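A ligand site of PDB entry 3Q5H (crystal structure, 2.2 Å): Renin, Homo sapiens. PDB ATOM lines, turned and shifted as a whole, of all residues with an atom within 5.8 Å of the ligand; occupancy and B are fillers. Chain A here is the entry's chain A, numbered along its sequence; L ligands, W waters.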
ATOM      1  N   THR A  18     -18.977 -10.076   9.292  1.00  0.00           N
ATOM      2  CA  THR A  18     -19.962 -10.997   8.767  1.00  0.00           C
ATOM      3  C   THR A  18     -20.154 -10.839   7.287  1.00  0.00           C
ATOM      4  O   THR A  18     -20.587 -11.771   6.631  1.00  0.00           O
ATOM      5  CB  THR A  18     -21.328 -10.819   9.483  1.00  0.00           C
ATOM      6  OG1 THR A  18     -21.797  -9.471   9.334  1.00  0.00           O
ATOM      7  CG2 THR A  18     -21.192 -11.131  10.965  1.00  0.00           C
ATOM      8  N   GLN A  19     -19.881  -9.662   6.716  1.00  0.00           N
ATOM      9  CA  GLN A  19     -19.919  -9.506   5.267  1.00  0.00           C
ATOM     10  C   GLN A  19     -18.623  -8.855   4.795  1.00  0.00           C
ATOM     11  O   GLN A  19     -18.216  -7.814   5.316  1.00  0.00           O
ATOM     12  CB  GLN A  19     -21.171  -8.696   4.787  1.00  0.00           C
ATOM     13  CG  GLN A  19     -22.575  -9.165   5.380  1.00  0.00           C
ATOM     14  CD  GLN A  19     -23.736  -8.292   4.958  1.00  0.00           C
ATOM     15  OE1 GLN A  19     -23.686  -7.637   3.935  1.00  0.00           O
ATOM     16  NE2 GLN A  19     -24.820  -8.296   5.752  1.00  0.00           N
ATOM     17  N   TYR A  20     -17.987  -9.464   3.814  1.00  0.00           N
ATOM     18  CA  TYR A  20     -16.837  -8.897   3.131  1.00  0.00           C
ATOM     19  C   TYR A  20     -17.126  -8.813   1.654  1.00  0.00           C
ATOM     20  O   TYR A  20     -17.554  -9.785   1.018  1.00  0.00           O
ATOM     21  CB  TYR A  20     -15.606  -9.787   3.312  1.00  0.00           C
ATOM     22  CG  TYR A  20     -15.149  -9.978   4.738  1.00  0.00           C
ATOM     23  CD1 TYR A  20     -15.867 -10.750   5.618  1.00  0.00           C
ATOM     24  CD2 TYR A  20     -13.996  -9.347   5.212  1.00  0.00           C
ATOM     25  CE1 TYR A  20     -15.448 -10.904   6.920  1.00  0.00           C
ATOM     26  CE2 TYR A  20     -13.568  -9.473   6.525  1.00  0.00           C
ATOM     27  CZ  TYR A  20     -14.267 -10.248   7.374  1.00  0.00           C
ATOM     28  OH  TYR A  20     -13.811 -10.458   8.675  1.00  0.00           O
ATOM     29  N   TYR A  21     -16.882  -7.628   1.087  1.00  0.00           N
ATOM     30  CA  TYR A  21     -17.226  -7.398  -0.256  1.00  0.00           C
ATOM     31  C   TYR A  21     -16.269  -6.424  -0.870  1.00  0.00           C
ATOM     32  O   TYR A  21     -15.596  -5.658  -0.171  1.00  0.00           O
ATOM     33  CB  TYR A  21     -18.661  -6.932  -0.363  1.00  0.00           C
ATOM     34  CG  TYR A  21     -18.964  -5.687   0.378  1.00  0.00           C
ATOM     35  CD1 TYR A  21     -18.831  -4.444  -0.253  1.00  0.00           C
ATOM     36  CD2 TYR A  21     -19.469  -5.733   1.664  1.00  0.00           C
ATOM     37  CE1 TYR A  21     -19.131  -3.255   0.436  1.00  0.00           C
ATOM     38  CE2 TYR A  21     -19.748  -4.563   2.388  1.00  0.00           C
ATOM     39  CZ  TYR A  21     -19.584  -3.327   1.775  1.00  0.00           C
ATOM     40  OH  TYR A  21     -19.898  -2.157   2.451  1.00  0.00           O
ATOM     41  N   VAL A  36     -19.810  -9.991  -3.081  1.00  0.00           N
ATOM     42  CA  VAL A  36     -19.143 -10.984  -2.255  1.00  0.00           C
ATOM     43  C   VAL A  36     -18.554 -11.984  -3.173  1.00  0.00           C
ATOM     44  O   VAL A  36     -19.234 -12.443  -4.102  1.00  0.00           O
ATOM     45  CB  VAL A  36     -20.174 -11.730  -1.392  1.00  0.00           C
ATOM     46  CG1 VAL A  36     -19.524 -12.842  -0.554  1.00  0.00           C
ATOM     47  CG2 VAL A  36     -20.871 -10.784  -0.516  1.00  0.00           C
ATOM     48  N   ASP A  38     -17.446 -15.576  -3.557  1.00  0.00           N
ATOM     49  CA  ASP A  38     -18.022 -16.731  -2.853  1.00  0.00           C
ATOM     50  C   ASP A  38     -17.460 -18.053  -3.402  1.00  0.00           C
ATOM     51  O   ASP A  38     -17.810 -18.463  -4.519  1.00  0.00           O
ATOM     52  CB  ASP A  38     -19.587 -16.659  -2.961  1.00  0.00           C
ATOM     53  CG  ASP A  38     -20.295 -17.836  -2.262  1.00  0.00           C
ATOM     54  OD1 ASP A  38     -19.697 -18.481  -1.368  1.00  0.00           O
ATOM     55  OD2 ASP A  38     -21.501 -18.129  -2.562  1.00  0.00           O
ATOM     56  N   THR A  39     -16.576 -18.731  -2.638  1.00  0.00           N
ATOM     57  CA  THR A  39     -16.058 -20.041  -3.131  1.00  0.00           C
ATOM     58  C   THR A  39     -17.119 -21.167  -3.093  1.00  0.00           C
ATOM     59  O   THR A  39     -16.942 -22.214  -3.687  1.00  0.00           O
ATOM     60  CB  THR A  39     -14.808 -20.492  -2.346  1.00  0.00           C
ATOM     61  OG1 THR A  39     -15.096 -20.448  -0.956  1.00  0.00           O
ATOM     62  CG2 THR A  39     -13.605 -19.617  -2.670  1.00  0.00           C
ATOM     63  N   GLY A  40     -18.201 -20.965  -2.333  1.00  0.00           N
ATOM     64  CA  GLY A  40     -19.261 -21.962  -2.291  1.00  0.00           C
ATOM     65  C   GLY A  40     -20.296 -21.799  -3.424  1.00  0.00           C
ATOM     66  O   GLY A  40     -21.327 -22.499  -3.413  1.00  0.00           O
ATOM     67  N   SER A  41     -20.068 -20.896  -4.381  1.00  0.00           N
ATOM     68  CA  SER A  41     -20.966 -20.846  -5.509  1.00  0.00           C
ATOM     69  C   SER A  41     -20.199 -20.416  -6.775  1.00  0.00           C
ATOM     70  O   SER A  41     -18.996 -20.082  -6.708  1.00  0.00           O
ATOM     71  CB  SER A  41     -22.167 -19.912  -5.225  1.00  0.00           C
ATOM     72  OG  SER A  41     -21.713 -18.566  -5.152  1.00  0.00           O
ATOM     73  N   TRP A  45     -23.743 -12.523 -10.402  1.00  0.00           N
ATOM     74  CA  TRP A  45     -24.995 -11.789 -10.653  1.00  0.00           C
ATOM     75  C   TRP A  45     -25.004 -10.437  -9.976  1.00  0.00           C
ATOM     76  O   TRP A  45     -24.395 -10.282  -8.949  1.00  0.00           O
ATOM     77  CB  TRP A  45     -26.286 -12.574 -10.227  1.00  0.00           C
ATOM     78  CG  TRP A  45     -26.390 -12.841  -8.706  1.00  0.00           C
ATOM     79  CD1 TRP A  45     -25.928 -13.937  -8.022  1.00  0.00           C
ATOM     80  CD2 TRP A  45     -27.010 -11.997  -7.727  1.00  0.00           C
ATOM     81  NE1 TRP A  45     -26.211 -13.824  -6.687  1.00  0.00           N
ATOM     82  CE2 TRP A  45     -26.859 -12.624  -6.469  1.00  0.00           C
ATOM     83  CE3 TRP A  45     -27.654 -10.739  -7.773  1.00  0.00           C
ATOM     84  CZ2 TRP A  45     -27.344 -12.067  -5.276  1.00  0.00           C
ATOM     85  CZ3 TRP A  45     -28.129 -10.165  -6.542  1.00  0.00           C
ATOM     86  CH2 TRP A  45     -27.951 -10.832  -5.340  1.00  0.00           C
ATOM     87  N   TYR A  83     -29.842 -20.010  -2.873  1.00  0.00           N
ATOM     88  CA  TYR A  83     -28.838 -20.047  -1.840  1.00  0.00           C
ATOM     89  C   TYR A  83     -29.518 -20.406  -0.521  1.00  0.00           C
ATOM     90  O   TYR A  83     -30.754 -20.419  -0.424  1.00  0.00           O
ATOM     91  CB  TYR A  83     -28.167 -18.683  -1.716  1.00  0.00           C
ATOM     92  CG  TYR A  83     -27.419 -18.176  -2.944  1.00  0.00           C
ATOM     93  CD1 TYR A  83     -26.097 -18.614  -3.234  1.00  0.00           C
ATOM     94  CD2 TYR A  83     -28.005 -17.231  -3.770  1.00  0.00           C
ATOM     95  CE1 TYR A  83     -25.412 -18.135  -4.331  1.00  0.00           C
ATOM     96  CE2 TYR A  83     -27.324 -16.755  -4.890  1.00  0.00           C
ATOM     97  CZ  TYR A  83     -26.026 -17.187  -5.163  1.00  0.00           C
ATOM     98  OH  TYR A  83     -25.366 -16.693  -6.271  1.00  0.00           O
ATOM     99  N   SER A  84     -28.704 -20.636   0.507  1.00  0.00           N
ATOM    100  CA  SER A  84     -29.168 -21.014   1.816  1.00  0.00           C
ATOM    101  C   SER A  84     -30.100 -19.943   2.311  1.00  0.00           C
ATOM    102  O   SER A  84     -30.987 -20.223   3.062  1.00  0.00           O
ATOM    103  CB  SER A  84     -27.992 -21.053   2.737  1.00  0.00           C
ATOM    104  OG  SER A  84     -27.439 -19.739   2.837  1.00  0.00           O
ATOM    105  N   THR A  85     -29.868 -18.711   1.887  1.00  0.00           N
ATOM    106  CA  THR A  85     -30.653 -17.521   2.295  1.00  0.00           C
ATOM    107  C   THR A  85     -31.939 -17.226   1.482  1.00  0.00           C
ATOM    108  O   THR A  85     -32.772 -16.364   1.845  1.00  0.00           O
ATOM    109  CB  THR A  85     -29.738 -16.251   2.124  1.00  0.00           C
ATOM    110  OG1 THR A  85     -29.178 -16.227   0.799  1.00  0.00           O
ATOM    111  CG2 THR A  85     -28.596 -16.234   3.113  1.00  0.00           C
ATOM    112  N   PRO A 118     -33.359 -12.327   2.341  1.00  0.00           N
ATOM    113  CA  PRO A 118     -32.682 -11.541   3.356  1.00  0.00           C
ATOM    114  C   PRO A 118     -31.825 -10.362   2.796  1.00  0.00           C
ATOM    115  O   PRO A 118     -31.012  -9.761   3.526  1.00  0.00           O
ATOM    116  CB  PRO A 118     -31.788 -12.626   3.985  1.00  0.00           C
ATOM    117  CG  PRO A 118     -31.243 -13.346   2.745  1.00  0.00           C
ATOM    118  CD  PRO A 118     -32.413 -13.295   1.719  1.00  0.00           C
ATOM    119  N   PHE A 119     -32.047 -10.038   1.523  1.00  0.00           N
ATOM    120  CA  PHE A 119     -31.230  -9.046   0.816  1.00  0.00           C
ATOM    121  C   PHE A 119     -31.399  -7.621   1.304  1.00  0.00           C
ATOM    122  O   PHE A 119     -30.590  -6.768   0.944  1.00  0.00           O
ATOM    123  CB  PHE A 119     -31.391  -9.118  -0.715  1.00  0.00           C
ATOM    124  CG  PHE A 119     -30.822 -10.365  -1.289  1.00  0.00           C
ATOM    125  CD1 PHE A 119     -29.476 -10.434  -1.579  1.00  0.00           C
ATOM    126  CD2 PHE A 119     -31.614 -11.485  -1.457  1.00  0.00           C
ATOM    127  CE1 PHE A 119     -28.907 -11.619  -2.071  1.00  0.00           C
ATOM    128  CE2 PHE A 119     -31.070 -12.714  -1.919  1.00  0.00           C
ATOM    129  CZ  PHE A 119     -29.708 -12.762  -2.240  1.00  0.00           C
ATOM    130  N   LEU A 121     -30.772  -7.086   4.152  1.00  0.00           N
ATOM    131  CA  LEU A 121     -29.720  -7.047   5.131  1.00  0.00           C
ATOM    132  C   LEU A 121     -28.366  -7.105   4.445  1.00  0.00           C
ATOM    133  O   LEU A 121     -27.389  -7.069   5.114  1.00  0.00           O
ATOM    134  CB  LEU A 121     -29.848  -8.227   6.102  1.00  0.00           C
ATOM    135  CG  LEU A 121     -31.013  -8.359   7.095  1.00  0.00           C
ATOM    136  CD1 LEU A 121     -30.933  -9.735   7.739  1.00  0.00           C
ATOM    137  CD2 LEU A 121     -30.971  -7.261   8.151  1.00  0.00           C
ATOM    138  N   ALA A 122     -28.329  -7.262   3.125  1.00  0.00           N
ATOM    139  CA  ALA A 122     -27.070  -7.364   2.370  1.00  0.00           C
ATOM    140  C   ALA A 122     -26.447  -5.981   2.210  1.00  0.00           C
ATOM    141  O   ALA A 122     -27.071  -5.026   1.643  1.00  0.00           O
ATOM    142  CB  ALA A 122     -27.347  -8.012   0.964  1.00  0.00           C
ATOM    143  N   PHE A 124     -23.958  -5.681   0.336  1.00  0.00           N
ATOM    144  CA  PHE A 124     -23.435  -5.781  -1.033  1.00  0.00           C
ATOM    145  C   PHE A 124     -24.577  -5.819  -2.034  1.00  0.00           C
ATOM    146  O   PHE A 124     -25.793  -6.024  -1.695  1.00  0.00           O
ATOM    147  CB  PHE A 124     -22.584  -7.082  -1.121  1.00  0.00           C
ATOM    148  CG  PHE A 124     -23.304  -8.289  -0.576  1.00  0.00           C
ATOM    149  CD1 PHE A 124     -23.277  -8.550   0.778  1.00  0.00           C
ATOM    150  CD2 PHE A 124     -24.038  -9.122  -1.429  1.00  0.00           C
ATOM    151  CE1 PHE A 124     -23.987  -9.621   1.279  1.00  0.00           C
ATOM    152  CE2 PHE A 124     -24.737 -10.201  -0.956  1.00  0.00           C
ATOM    153  CZ  PHE A 124     -24.743 -10.473   0.377  1.00  0.00           C
ATOM    154  N   VAL A 127     -23.081 -11.116  -6.253  1.00  0.00           N
ATOM    155  CA  VAL A 127     -22.181 -12.190  -5.852  1.00  0.00           C
ATOM    156  C   VAL A 127     -21.339 -12.520  -7.060  1.00  0.00           C
ATOM    157  O   VAL A 127     -21.842 -12.532  -8.178  1.00  0.00           O
ATOM    158  CB  VAL A 127     -22.923 -13.435  -5.415  1.00  0.00           C
ATOM    159  CG1 VAL A 127     -21.920 -14.595  -5.083  1.00  0.00           C
ATOM    160  CG2 VAL A 127     -23.833 -13.140  -4.176  1.00  0.00           C
ATOM    161  N   TYR A 162      -8.992 -11.983   5.207  1.00  0.00           N
ATOM    162  CA  TYR A 162     -10.089 -11.302   5.830  1.00  0.00           C
ATOM    163  C   TYR A 162      -9.587 -10.761   7.158  1.00  0.00           C
ATOM    164  O   TYR A 162      -9.124 -11.496   7.934  1.00  0.00           O
ATOM    165  CB  TYR A 162     -11.238 -12.272   6.061  1.00  0.00           C
ATOM    166  CG  TYR A 162     -12.176 -12.606   4.927  1.00  0.00           C
ATOM    167  CD1 TYR A 162     -12.204 -11.870   3.787  1.00  0.00           C
ATOM    168  CD2 TYR A 162     -13.056 -13.658   5.017  1.00  0.00           C
ATOM    169  CE1 TYR A 162     -13.034 -12.180   2.788  1.00  0.00           C
ATOM    170  CE2 TYR A 162     -13.885 -13.972   4.009  1.00  0.00           C
ATOM    171  CZ  TYR A 162     -13.873 -13.233   2.895  1.00  0.00           C
ATOM    172  OH  TYR A 162     -14.684 -13.519   1.886  1.00  0.00           O
ATOM    173  N   LEU A 224     -16.095 -27.821   3.574  1.00  0.00           N
ATOM    174  CA  LEU A 224     -16.111 -26.845   2.496  1.00  0.00           C
ATOM    175  C   LEU A 224     -15.278 -25.592   2.929  1.00  0.00           C
ATOM    176  O   LEU A 224     -15.372 -25.163   4.074  1.00  0.00           O
ATOM    177  CB  LEU A 224     -17.582 -26.498   2.185  1.00  0.00           C
ATOM    178  CG  LEU A 224     -17.833 -25.659   0.946  1.00  0.00           C
ATOM    179  CD1 LEU A 224     -17.431 -26.511  -0.235  1.00  0.00           C
ATOM    180  CD2 LEU A 224     -19.313 -25.157   0.793  1.00  0.00           C
ATOM    181  N   ASP A 226     -15.287 -21.905   2.466  1.00  0.00           N
ATOM    182  CA  ASP A 226     -16.409 -21.130   1.918  1.00  0.00           C
ATOM    183  C   ASP A 226     -16.279 -19.700   2.281  1.00  0.00           C
ATOM    184  O   ASP A 226     -16.717 -19.289   3.350  1.00  0.00           O
ATOM    185  CB  ASP A 226     -17.796 -21.622   2.401  1.00  0.00           C
ATOM    186  CG  ASP A 226     -18.899 -21.077   1.509  1.00  0.00           C
ATOM    187  OD1 ASP A 226     -18.655 -20.048   0.794  1.00  0.00           O
ATOM    188  OD2 ASP A 226     -19.971 -21.673   1.419  1.00  0.00           O
ATOM    189  N   THR A 227     -15.646 -18.962   1.409  1.00  0.00           N
ATOM    190  CA  THR A 227     -15.384 -17.526   1.605  1.00  0.00           C
ATOM    191  C   THR A 227     -16.669 -16.670   1.582  1.00  0.00           C
ATOM    192  O   THR A 227     -16.642 -15.504   1.963  1.00  0.00           O
ATOM    193  CB  THR A 227     -14.479 -17.004   0.479  1.00  0.00           C
ATOM    194  OG1 THR A 227     -15.135 -17.149  -0.805  1.00  0.00           O
ATOM    195  CG2 THR A 227     -13.153 -17.720   0.495  1.00  0.00           C
ATOM    196  N   GLY A 228     -17.799 -17.230   1.153  1.00  0.00           N
ATOM    197  CA  GLY A 228     -19.090 -16.499   1.234  1.00  0.00           C
ATOM    198  C   GLY A 228     -19.855 -16.811   2.532  1.00  0.00           C
ATOM    199  O   GLY A 228     -20.988 -16.328   2.766  1.00  0.00           O
ATOM    200  N   ALA A 229     -19.276 -17.664   3.380  1.00  0.00           N
ATOM    201  CA  ALA A 229     -19.966 -17.986   4.657  1.00  0.00           C
ATOM    202  C   ALA A 229     -19.455 -17.104   5.818  1.00  0.00           C
ATOM    203  O   ALA A 229     -18.235 -16.927   5.998  1.00  0.00           O
ATOM    204  CB  ALA A 229     -19.787 -19.514   5.006  1.00  0.00           C
ATOM    205  N   SER A 230     -20.318 -16.536   6.625  1.00  0.00           N
ATOM    206  CA  SER A 230     -19.800 -15.625   7.683  1.00  0.00           C
ATOM    207  C   SER A 230     -19.140 -16.444   8.793  1.00  0.00           C
ATOM    208  O   SER A 230     -18.003 -16.141   9.203  1.00  0.00           O
ATOM    209  CB  SER A 230     -20.896 -14.815   8.309  1.00  0.00           C
ATOM    210  OG  SER A 230     -21.686 -14.143   7.335  1.00  0.00           O
ATOM    211  N   HIS A 301     -22.544 -21.774  13.601  1.00  0.00           N
ATOM    212  CA  HIS A 301     -23.956 -22.104  13.653  1.00  0.00           C
ATOM    213  C   HIS A 301     -24.161 -23.406  12.870  1.00  0.00           C
ATOM    214  O   HIS A 301     -23.209 -23.895  12.270  1.00  0.00           O
ATOM    215  CB  HIS A 301     -24.811 -20.936  13.066  1.00  0.00           C
ATOM    216  CG  HIS A 301     -24.585 -20.704  11.610  1.00  0.00           C
ATOM    217  ND1 HIS A 301     -25.435 -19.933  10.838  1.00  0.00           N
ATOM    218  CD2 HIS A 301     -23.612 -21.139  10.762  1.00  0.00           C
ATOM    219  CE1 HIS A 301     -24.997 -19.900   9.595  1.00  0.00           C
ATOM    220  NE2 HIS A 301     -23.872 -20.595   9.533  1.00  0.00           N
ATOM    221  N   MET A 303     -25.650 -25.491   9.788  1.00  0.00           N
ATOM    222  CA  MET A 303     -26.251 -25.439   8.458  1.00  0.00           C
ATOM    223  C   MET A 303     -26.229 -26.860   7.861  1.00  0.00           C
ATOM    224  O   MET A 303     -25.150 -27.373   7.624  1.00  0.00           O
ATOM    225  CB  MET A 303     -25.504 -24.477   7.556  1.00  0.00           C
ATOM    226  CG  MET A 303     -26.493 -23.705   6.588  1.00  0.00           C
ATOM    227  SD  MET A 303     -25.663 -22.363   5.653  1.00  0.00           S
ATOM    228  CE  MET A 303     -24.728 -23.415   4.589  1.00  0.00           C
ATOM    229  N   ALA A 317     -15.728 -17.194   7.333  1.00  0.00           N
ATOM    230  CA  ALA A 317     -14.850 -16.057   7.795  1.00  0.00           C
ATOM    231  C   ALA A 317     -14.277 -16.226   9.201  1.00  0.00           C
ATOM    232  O   ALA A 317     -13.157 -15.785   9.441  1.00  0.00           O
ATOM    233  CB  ALA A 317     -15.543 -14.711   7.677  1.00  0.00           C
HETATM  234  C1  LIG L   1     -24.463 -13.902   4.669  1.00  0.00           C
HETATM  235  N1  LIG L   1     -20.776 -13.740   3.039  1.00  0.00           N
HETATM  236  O1  LIG L   1     -26.395 -15.519   0.351  1.00  0.00           O
HETATM  237  C2  LIG L   1     -17.539 -13.771   4.545  1.00  0.00           C
HETATM  238  O2  LIG L   1     -18.690 -14.327   3.910  1.00  0.00           O
HETATM  239  C3  LIG L   1     -25.595 -12.994   4.436  1.00  0.00           C
HETATM  240  O3  LIG L   1     -23.619 -13.613   3.561  1.00  0.00           O
HETATM  241  C4  LIG L   1     -26.244 -12.922   3.180  1.00  0.00           C
HETATM  242  C5  LIG L   1     -25.995 -12.153   5.476  1.00  0.00           C
HETATM  243  C6  LIG L   1     -27.270 -12.010   3.002  1.00  0.00           C
HETATM  244  C7  LIG L   1     -27.026 -11.260   5.273  1.00  0.00           C
HETATM  245  C8  LIG L   1     -27.671 -11.186   4.039  1.00  0.00           C
HETATM  246  C9  LIG L   1     -19.600 -13.337   3.427  1.00  0.00           C
HETATM  247 CL1  LIG L   1     -28.173 -11.920   1.450  1.00  0.00          CL
HETATM  248  C10 LIG L   1     -23.247 -18.498   1.328  1.00  0.00           C
HETATM  249  C11 LIG L   1     -22.127 -19.537   1.378  1.00  0.00           C
HETATM  250  C12 LIG L   1     -23.021 -17.361   0.345  1.00  0.00           C
HETATM  251  N2  LIG L   1     -21.608 -19.918   0.035  1.00  0.00           N
HETATM  252  O4  LIG L   1     -19.279 -12.155   3.397  1.00  0.00           O
HETATM  253  C13 LIG L   1     -24.052 -16.230   0.428  1.00  0.00           C
HETATM  254  C14 LIG L   1     -23.753 -15.250  -0.704  1.00  0.00           C
HETATM  255  C15 LIG L   1     -24.835 -14.164  -0.773  1.00  0.00           C
HETATM  256  C16 LIG L   1     -26.300 -14.636  -0.724  1.00  0.00           C
HETATM  257  C17 LIG L   1     -25.496 -16.672   0.263  1.00  0.00           C
HETATM  258  N3  LIG L   1     -23.431 -17.854   2.603  1.00  0.00           N
HETATM  259  C18 LIG L   1     -24.216 -18.356   3.555  1.00  0.00           C
HETATM  260  O5  LIG L   1     -24.823 -19.442   3.391  1.00  0.00           O
HETATM  261  N4  LIG L   1     -24.312 -17.634   4.678  1.00  0.00           N
HETATM  262  C19 LIG L   1     -26.416 -17.077   5.737  1.00  0.00           C
HETATM  263  C20 LIG L   1     -25.997 -15.625   5.631  1.00  0.00           C
HETATM  264  C21 LIG L   1     -24.871 -15.357   4.588  1.00  0.00           C
HETATM  265  C22 LIG L   1     -23.678 -16.318   4.888  1.00  0.00           C
HETATM  266  C23 LIG L   1     -25.163 -18.044   5.779  1.00  0.00           C
HETATM  267  C24 LIG L   1     -22.463 -20.762  -0.793  1.00  0.00           C
HETATM  268  C25 LIG L   1     -22.708 -12.527   3.727  1.00  0.00           C
HETATM  269  C26 LIG L   1     -21.705 -12.752   2.577  1.00  0.00           C
HETATM  270  O   HOH W   1     -24.536 -22.033   2.113  1.00  0.00           O
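An oxygen (O2) of the ligand lies within hydrogen-bond range of the backbone NH of Ala 229, at 3.4 Å.
The backbone carbonyl oxygen (O) of Gly 228 sits at hydrogen-bond distance from a nitrogen (N1) of the ligand, 2.6 Å away.
An oxygen (O4) of the ligand is in hydrogen-bond range of the backbone NH of Tyr 20, 3.0 Å away.
OD2 of Asp 226 is in salt-bridge range of N2 of the ligand, at 2.8 Å.
A nitrogen (N2) of the ligand lies within salt-bridge range of the side-chain carboxylate of Asp 38, 2.8 Å away.
The side-chain hydroxyl (OG) of Ser 84 is in hydrogen-bond range of an oxygen (O5) of the ligand (2.7 Å).
O1 of the ligand is in hydrogen-bond range of OG1 of Thr 85 (2.9 Å).
Water W1 bridges an oxygen (O5) of the ligand (2.9 Å) and the side-chain sulfur of Met 303 (3.7 Å).
The backbone NH of Gly 228 is in hydrogen-bond range of the side-chain carboxylate of Asp 226 (3.0 Å).
The backbone NH of Gly 40 lies within hydrogen-bond range of the side-chain carboxylate of Asp 226 (3.3 Å).
The side-chain hydroxyl (OG1) of Thr 227 lies within hydrogen-bond range of the backbone NH (N) of Thr 39, at 2.8 Å.
NE1 of Trp 45 is in hydrogen-bond range of OH of Tyr 83 (3.0 Å).
The side-chain hydroxyl of Tyr 162 sits at hydrogen-bond distance from the backbone carbonyl oxygen of Thr 227 (2.8 Å).
The backbone carbonyl oxygen (O) of Val 127 sits at hydrogen-bond distance from the backbone NH (N) of Trp 45 (2.9 Å).
OD1 of Asp 38 lies within hydrogen-bond range of N of Gly 40, at 3.1 Å.
O of Thr 18 lies within hydrogen-bond range of OG of Ser 230 (2.7 Å).
The backbone carbonyl oxygen of Thr 227 sits close to an oxygen (O2) of the ligand (3.1 Å).
An oxygen (O5) of the ligand lies close to the side-chain sulfur (SD) of Met 303, 3.8 Å away.
Merely in contact with the ligand: Thr 18 (3.5 Å), Gln 19 (3.3 Å), Val 36 (3.8 Å), Gly 40 (3.3 Å), Tyr 83 (3.9 Å), Pro 118 (3.6 Å), Phe 119 (3.6 Å), Phe 124 (3.9 Å), Val 127 (3.7 Å), Tyr 162 (3.7 Å), Ser 230 (3.8 Å) and Ala 317 (3.8 Å).
Within 4 Å of the ligand: Thr 18, Gln 19, Tyr 20, Val 36, Asp 38, Gly 40, Tyr 83, Ser 84, Thr 85, Pro 118, Phe 119, Phe 124, Val 127, Tyr 162, Asp 226, Thr 227, Gly 228, Ala 229, Ser 230, Met 303 and Ala 317.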
